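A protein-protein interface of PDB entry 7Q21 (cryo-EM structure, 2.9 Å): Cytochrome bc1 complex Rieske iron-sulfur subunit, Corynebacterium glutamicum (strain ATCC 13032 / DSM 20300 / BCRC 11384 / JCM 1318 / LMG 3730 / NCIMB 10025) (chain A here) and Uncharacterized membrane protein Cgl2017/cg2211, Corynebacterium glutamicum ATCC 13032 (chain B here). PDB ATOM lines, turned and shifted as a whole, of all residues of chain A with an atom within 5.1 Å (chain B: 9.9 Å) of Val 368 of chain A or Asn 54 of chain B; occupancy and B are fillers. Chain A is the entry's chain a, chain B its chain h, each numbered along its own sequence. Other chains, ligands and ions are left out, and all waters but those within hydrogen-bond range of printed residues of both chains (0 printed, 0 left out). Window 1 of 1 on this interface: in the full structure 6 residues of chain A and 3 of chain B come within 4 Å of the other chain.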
ATOM      1  N   ARG A 349       1.496  13.382 -18.947  1.00  0.00           N
ATOM      2  CA  ARG A 349       0.546  13.759 -17.915  1.00  0.00           C
ATOM      3  C   ARG A 349      -0.715  14.275 -18.597  1.00  0.00           C
ATOM      4  O   ARG A 349      -0.638  14.934 -19.636  1.00  0.00           O
ATOM      5  CB  ARG A 349       1.113  14.836 -16.989  1.00  0.00           C
ATOM      6  CG  ARG A 349       2.103  14.334 -15.947  1.00  0.00           C
ATOM      7  CD  ARG A 349       2.410  15.325 -14.849  1.00  0.00           C
ATOM      8  NE  ARG A 349       2.993  16.598 -15.256  1.00  0.00           N
ATOM      9  CZ  ARG A 349       4.294  16.855 -15.341  1.00  0.00           C
ATOM     10  NH1 ARG A 349       4.702  18.058 -15.710  1.00  0.00           N
ATOM     11  NH2 ARG A 349       5.183  15.931 -15.014  1.00  0.00           N
ATOM     12  N   GLN A 358      -3.262  16.619 -12.408  1.00  0.00           N
ATOM     13  CA  GLN A 358      -2.404  15.942 -13.368  1.00  0.00           C
ATOM     14  C   GLN A 358      -2.444  14.446 -13.083  1.00  0.00           C
ATOM     15  O   GLN A 358      -2.025  14.004 -12.018  1.00  0.00           O
ATOM     16  CB  GLN A 358      -0.966  16.461 -13.311  1.00  0.00           C
ATOM     17  CG  GLN A 358      -0.775  17.833 -13.947  1.00  0.00           C
ATOM     18  CD  GLN A 358      -0.025  18.787 -13.050  1.00  0.00           C
ATOM     19  OE1 GLN A 358       1.056  18.486 -12.547  1.00  0.00           O
ATOM     20  NE2 GLN A 358      -0.605  19.952 -12.808  1.00  0.00           N
ATOM     21  N   PHE A 359      -2.955  13.681 -14.052  1.00  0.00           N
ATOM     22  CA  PHE A 359      -3.011  12.232 -13.958  1.00  0.00           C
ATOM     23  C   PHE A 359      -1.876  11.646 -14.784  1.00  0.00           C
ATOM     24  O   PHE A 359      -1.702  12.007 -15.944  1.00  0.00           O
ATOM     25  CB  PHE A 359      -4.364  11.720 -14.454  1.00  0.00           C
ATOM     26  CG  PHE A 359      -5.554  12.320 -13.751  1.00  0.00           C
ATOM     27  CD1 PHE A 359      -6.032  11.777 -12.564  1.00  0.00           C
ATOM     28  CD2 PHE A 359      -6.197  13.435 -14.274  1.00  0.00           C
ATOM     29  CE1 PHE A 359      -7.128  12.336 -11.919  1.00  0.00           C
ATOM     30  CE2 PHE A 359      -7.294  13.991 -13.627  1.00  0.00           C
ATOM     31  CZ  PHE A 359      -7.761  13.439 -12.453  1.00  0.00           C
ATOM     32  N   ASP A 360      -1.111  10.736 -14.172  1.00  0.00           N
ATOM     33  CA  ASP A 360      -0.023  10.055 -14.860  1.00  0.00           C
ATOM     34  C   ASP A 360      -0.610   9.120 -15.916  1.00  0.00           C
ATOM     35  O   ASP A 360      -1.772   8.757 -15.818  1.00  0.00           O
ATOM     36  CB  ASP A 360       0.925   9.398 -13.854  1.00  0.00           C
ATOM     37  CG  ASP A 360       2.358   9.314 -14.351  1.00  0.00           C
ATOM     38  OD1 ASP A 360       2.634   9.825 -15.460  1.00  0.00           O
ATOM     39  OD2 ASP A 360       3.195   8.743 -13.624  1.00  0.00           O
ATOM     40  N   LYS A 366      -2.860   7.567 -12.108  1.00  0.00           N
ATOM     41  CA  LYS A 366      -2.754   8.046 -10.738  1.00  0.00           C
ATOM     42  C   LYS A 366      -2.486   9.552 -10.730  1.00  0.00           C
ATOM     43  O   LYS A 366      -1.575  10.014 -11.415  1.00  0.00           O
ATOM     44  CB  LYS A 366      -1.681   7.259  -9.981  1.00  0.00           C
ATOM     45  CG  LYS A 366      -1.714   7.406  -8.468  1.00  0.00           C
ATOM     46  CD  LYS A 366      -0.496   6.803  -7.802  1.00  0.00           C
ATOM     47  CE  LYS A 366      -0.507   6.947  -6.296  1.00  0.00           C
ATOM     48  NZ  LYS A 366      -1.526   6.071  -5.667  1.00  0.00           N
ATOM     49  N   PRO A 367      -3.275  10.363  -9.982  1.00  0.00           N
ATOM     50  CA  PRO A 367      -3.050  11.810  -9.909  1.00  0.00           C
ATOM     51  C   PRO A 367      -1.739  12.150  -9.204  1.00  0.00           C
ATOM     52  O   PRO A 367      -1.332  11.460  -8.271  1.00  0.00           O
ATOM     53  CB  PRO A 367      -4.232  12.360  -9.098  1.00  0.00           C
ATOM     54  CG  PRO A 367      -5.225  11.234  -9.030  1.00  0.00           C
ATOM     55  CD  PRO A 367      -4.439   9.946  -9.185  1.00  0.00           C
ATOM     56  N   VAL A 368      -1.081  13.208  -9.684  1.00  0.00           N
ATOM     57  CA  VAL A 368       0.214  13.627  -9.170  1.00  0.00           C
ATOM     58  C   VAL A 368       0.190  15.123  -8.864  1.00  0.00           C
ATOM     59  O   VAL A 368       1.235  15.716  -8.589  1.00  0.00           O
ATOM     60  CB  VAL A 368       1.368  13.253 -10.126  1.00  0.00           C
ATOM     61  CG1 VAL A 368       1.551  11.748 -10.265  1.00  0.00           C
ATOM     62  CG2 VAL A 368       1.227  13.907 -11.493  1.00  0.00           C
ATOM     63  N   PHE A 369      -1.004  15.723  -8.924  1.00  0.00           N
ATOM     64  CA  PHE A 369      -1.210  17.118  -8.570  1.00  0.00           C
ATOM     65  C   PHE A 369      -2.705  17.421  -8.540  1.00  0.00           C
ATOM     66  O   PHE A 369      -3.501  16.654  -9.076  1.00  0.00           O
ATOM     67  CB  PHE A 369      -0.492  18.045  -9.555  1.00  0.00           C
ATOM     68  CG  PHE A 369      -0.200  19.425  -9.026  1.00  0.00           C
ATOM     69  CD1 PHE A 369       0.954  19.674  -8.294  1.00  0.00           C
ATOM     70  CD2 PHE A 369      -1.069  20.483  -9.275  1.00  0.00           C
ATOM     71  CE1 PHE A 369       1.226  20.949  -7.812  1.00  0.00           C
ATOM     72  CE2 PHE A 369      -0.801  21.753  -8.782  1.00  0.00           C
ATOM     73  CZ  PHE A 369       0.348  21.985  -8.055  1.00  0.00           C
ATOM     74  N   GLY A 370      -3.064  18.528  -7.883  1.00  0.00           N
ATOM     75  CA  GLY A 370      -4.422  19.047  -7.910  1.00  0.00           C
ATOM     76  C   GLY A 370      -5.345  18.344  -6.915  1.00  0.00           C
ATOM     77  O   GLY A 370      -4.902  17.515  -6.121  1.00  0.00           O
ATOM     78  N   ALA A 372      -7.793  16.132  -7.275  1.00  0.00           N
ATOM     79  CA  ALA A 372      -8.222  14.776  -7.576  1.00  0.00           C
ATOM     80  C   ALA A 372      -7.443  13.784  -6.719  1.00  0.00           C
ATOM     81  O   ALA A 372      -6.226  13.898  -6.588  1.00  0.00           O
ATOM     82  CB  ALA A 372      -8.064  14.491  -9.048  1.00  0.00           C
ATOM     83  N   ALA A 373      -8.162  12.802  -6.161  1.00  0.00           N
ATOM     84  CA  ALA A 373      -7.582  11.850  -5.226  1.00  0.00           C
ATOM     85  C   ALA A 373      -7.594  10.432  -5.791  1.00  0.00           C
ATOM     86  O   ALA A 373      -6.779   9.605  -5.383  1.00  0.00           O
ATOM     87  CB  ALA A 373      -8.305  11.920  -3.905  1.00  0.00           C
ATOM     88  N   GLY B  49       0.149  20.704   7.315  1.00  0.00           N
ATOM     89  CA  GLY B  49      -0.837  19.801   6.743  1.00  0.00           C
ATOM     90  C   GLY B  49      -0.859  19.827   5.218  1.00  0.00           C
ATOM     91  O   GLY B  49      -1.466  18.948   4.610  1.00  0.00           O
ATOM     92  N   TYR B  50      -0.209  20.831   4.613  1.00  0.00           N
ATOM     93  CA  TYR B  50      -0.130  20.927   3.162  1.00  0.00           C
ATOM     94  C   TYR B  50       0.746  19.828   2.567  1.00  0.00           C
ATOM     95  O   TYR B  50       0.635  19.533   1.380  1.00  0.00           O
ATOM     96  CB  TYR B  50       0.370  22.300   2.713  1.00  0.00           C
ATOM     97  CG  TYR B  50      -0.688  23.368   2.618  1.00  0.00           C
ATOM     98  CD1 TYR B  50      -0.339  24.710   2.638  1.00  0.00           C
ATOM     99  CD2 TYR B  50      -2.033  23.045   2.510  1.00  0.00           C
ATOM    100  CE1 TYR B  50      -1.300  25.707   2.549  1.00  0.00           C
ATOM    101  CE2 TYR B  50      -3.006  24.029   2.418  1.00  0.00           C
ATOM    102  CZ  TYR B  50      -2.638  25.365   2.438  1.00  0.00           C
ATOM    103  OH  TYR B  50      -3.589  26.339   2.350  1.00  0.00           O
ATOM    104  N   ASN B  51       1.581  19.198   3.406  1.00  0.00           N
ATOM    105  CA  ASN B  51       2.551  18.204   2.959  1.00  0.00           C
ATOM    106  C   ASN B  51       1.890  16.845   2.718  1.00  0.00           C
ATOM    107  O   ASN B  51       2.567  15.852   2.448  1.00  0.00           O
ATOM    108  CB  ASN B  51       3.690  18.059   3.972  1.00  0.00           C
ATOM    109  CG  ASN B  51       4.579  19.280   4.055  1.00  0.00           C
ATOM    110  OD1 ASN B  51       5.164  19.686   3.058  1.00  0.00           O
ATOM    111  ND2 ASN B  51       4.653  19.889   5.231  1.00  0.00           N
ATOM    112  N   PHE B  52       0.559  16.784   2.842  1.00  0.00           N
ATOM    113  CA  PHE B  52      -0.190  15.540   2.755  1.00  0.00           C
ATOM    114  C   PHE B  52      -1.149  15.575   1.567  1.00  0.00           C
ATOM    115  O   PHE B  52      -2.326  15.228   1.688  1.00  0.00           O
ATOM    116  CB  PHE B  52      -0.884  15.221   4.087  1.00  0.00           C
ATOM    117  CG  PHE B  52       0.049  15.026   5.254  1.00  0.00           C
ATOM    118  CD1 PHE B  52       0.019  15.893   6.341  1.00  0.00           C
ATOM    119  CD2 PHE B  52       0.944  13.960   5.288  1.00  0.00           C
ATOM    120  CE1 PHE B  52       0.875  15.713   7.421  1.00  0.00           C
ATOM    121  CE2 PHE B  52       1.799  13.781   6.367  1.00  0.00           C
ATOM    122  CZ  PHE B  52       1.761  14.656   7.433  1.00  0.00           C
ATOM    123  N   GLY B  53      -0.635  15.976   0.399  1.00  0.00           N
ATOM    124  CA  GLY B  53      -1.357  15.907  -0.864  1.00  0.00           C
ATOM    125  C   GLY B  53      -0.858  14.749  -1.724  1.00  0.00           C
ATOM    126  O   GLY B  53      -0.492  13.710  -1.181  1.00  0.00           O
ATOM    127  N   ASN B  54      -0.830  14.947  -3.045  1.00  0.00           N
ATOM    128  CA  ASN B  54      -0.433  13.897  -3.972  1.00  0.00           C
ATOM    129  C   ASN B  54       0.790  14.326  -4.779  1.00  0.00           C
ATOM    130  O   ASN B  54       1.300  13.531  -5.568  1.00  0.00           O
ATOM    131  CB  ASN B  54      -1.578  13.473  -4.902  1.00  0.00           C
ATOM    132  CG  ASN B  54      -2.355  14.651  -5.449  1.00  0.00           C
ATOM    133  OD1 ASN B  54      -1.899  15.791  -5.379  1.00  0.00           O
ATOM    134  ND2 ASN B  54      -3.535  14.390  -5.984  1.00  0.00           N
ATOM    135  N   HIS B  55       1.237  15.571  -4.573  1.00  0.00           N
ATOM    136  CA  HIS B  55       2.331  16.169  -5.324  1.00  0.00           C
ATOM    137  C   HIS B  55       3.587  15.320  -5.161  1.00  0.00           C
ATOM    138  O   HIS B  55       3.923  14.891  -4.061  1.00  0.00           O
ATOM    139  CB  HIS B  55       2.549  17.631  -4.902  1.00  0.00           C
ATOM    140  CG  HIS B  55       2.719  17.803  -3.429  1.00  0.00           C
ATOM    141  ND1 HIS B  55       1.639  17.993  -2.589  1.00  0.00           N
ATOM    142  CD2 HIS B  55       3.817  17.793  -2.643  1.00  0.00           C
ATOM    143  CE1 HIS B  55       2.063  18.076  -1.352  1.00  0.00           C
ATOM    144  NE2 HIS B  55       3.395  17.978  -1.354  1.00  0.00           N
ATOM    145  N   LYS B  56       4.254  15.067  -6.291  1.00  0.00           N
ATOM    146  CA  LYS B  56       5.444  14.233  -6.335  1.00  0.00           C
ATOM    147  C   LYS B  56       6.703  15.072  -6.120  1.00  0.00           C
ATOM    148  O   LYS B  56       7.712  14.540  -5.665  1.00  0.00           O
ATOM    149  CB  LYS B  56       5.505  13.469  -7.660  1.00  0.00           C
ATOM    150  CG  LYS B  56       5.212  11.980  -7.562  1.00  0.00           C
ATOM    151  CD  LYS B  56       5.133  11.306  -8.917  1.00  0.00           C
ATOM    152  CE  LYS B  56       4.596   9.892  -8.847  1.00  0.00           C
ATOM    153  NZ  LYS B  56       4.376   9.309 -10.195  1.00  0.00           N
ATOM    154  N   GLY B  57       6.631  16.365  -6.463  1.00  0.00           N
ATOM    155  CA  GLY B  57       7.756  17.281  -6.373  1.00  0.00           C
ATOM    156  C   GLY B  57       8.102  17.639  -4.929  1.00  0.00           C
ATOM    157  O   GLY B  57       7.284  17.491  -4.023  1.00  0.00           O
ATOM    158  N   HIS B  58       9.340  18.114  -4.741  1.00  0.00           N
ATOM    159  CA  HIS B  58       9.862  18.435  -3.422  1.00  0.00           C
ATOM    160  C   HIS B  58      10.339  19.883  -3.332  1.00  0.00           C
ATOM    161  O   HIS B  58      10.911  20.277  -2.320  1.00  0.00           O
ATOM    162  CB  HIS B  58      10.958  17.446  -3.010  1.00  0.00           C
ATOM    163  CG  HIS B  58      10.415  16.178  -2.444  1.00  0.00           C
ATOM    164  ND1 HIS B  58       9.544  16.157  -1.365  1.00  0.00           N
ATOM    165  CD2 HIS B  58      10.669  14.888  -2.747  1.00  0.00           C
ATOM    166  CE1 HIS B  58       9.249  14.910  -1.065  1.00  0.00           C
ATOM    167  NE2 HIS B  58       9.928  14.110  -1.898  1.00  0.00           N
ATOM    168  N   GLU B  60       8.243  22.434  -3.587  1.00  0.00           N
ATOM    169  CA  GLU B  60       7.157  23.092  -2.879  1.00  0.00           C
ATOM    170  C   GLU B  60       7.221  22.801  -1.382  1.00  0.00           C
ATOM    171  O   GLU B  60       6.827  23.650  -0.596  1.00  0.00           O
ATOM    172  CB  GLU B  60       5.796  22.729  -3.465  1.00  0.00           C
ATOM    173  CG  GLU B  60       5.557  21.233  -3.616  1.00  0.00           C
ATOM    174  CD  GLU B  60       5.739  20.701  -5.031  1.00  0.00           C
ATOM    175  OE1 GLU B  60       6.403  21.376  -5.851  1.00  0.00           O
ATOM    176  OE2 GLU B  60       5.208  19.612  -5.319  1.00  0.00           O
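The backbone carbonyl oxygen (O) of Gly 370 of chain A sits at hydrogen-bond distance from the side-chain amide nitrogen (ND2) of Asn 54 of chain B, at 3.4 Å.
The side-chain amide nitrogen of Asn 54 of chain B is in hydrogen-bond range of the backbone carbonyl oxygen of Ala 372 of chain A.
NZ of Lys 56 of chain B lies within salt-bridge range of OD2 of Asp 360 of chain A, 3.7 Å away.
The backbone NH (N) of Asp 360 of chain A is in hydrogen-bond range of the backbone carbonyl oxygen (O) of Lys 366 of chain A.
The backbone carbonyl oxygen (O) of Phe 369 of chain A is in hydrogen-bond range of the backbone NH (N) of Gln 358 of chain A, at 3.3 Å.
The backbone carbonyl oxygen (O) of Gln 358 of chain A sits at hydrogen-bond distance from the backbone NH (N) of Val 368 of chain A.
ND2 of Asn 54 of chain B touches CB of Pro 367 of chain A, at 3.8 Å.
Val 368 of chain A touches Asn 54 of chain B (O to O, 3.7 Å).
Val 368 of chain A touches His 55 of chain B.
Val 368 of chain A touches Lys 56 of chain B.
Phe 369 of chain A touches Asn 54 of chain B (CA to OD1, 3.5 Å).
Val 368 of chain A touches just these residues of chain B: Asn 54 (3.7 Å), His 55 (3.5 Å) and Lys 56 (3.7 Å).
Asn 54 of chain B touches just these residues of chain A: Pro 367, Val 368, Phe 369, Gly 370 and Ala 372.
Pro 367 of chain A touches one residue of chain B.
Ala 372 of chain A touches just one residue of chain B: Asn 54 (2.8 Å).
No residue of chain B comes within 4 Å of Ala 373 of chain A.
Of the printed residues of chain B, Asp 360 of chain A touches Lys 56.
Of the printed residues of chain A, Lys 56 of chain B touches Asp 360 and Val 368.
Of the printed residues of chain A, His 55 of chain B touches Val 368 (3.5 Å).
Printed residues of chain B within 4 Å of Phe 369 of chain A: Asn 54 (3.5 Å).
The nearest residue of chain B that does not touch Val 368 of chain A is Gly 57 of chain B (5.8 Å).
Hydrophobic or aromatic side chains of chain A within 4 Å of the printed part of chain B: Pro 367 and Val 368.
Among the printed residues, 8 pairs touch across the chains.
Among the printed residues, Asp or Glu carboxylates within 4 Å of a Lys or Arg side-chain nitrogen of the other chain: Asp 360 of chain A with Lys 56 of chain B (3.7 Å).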
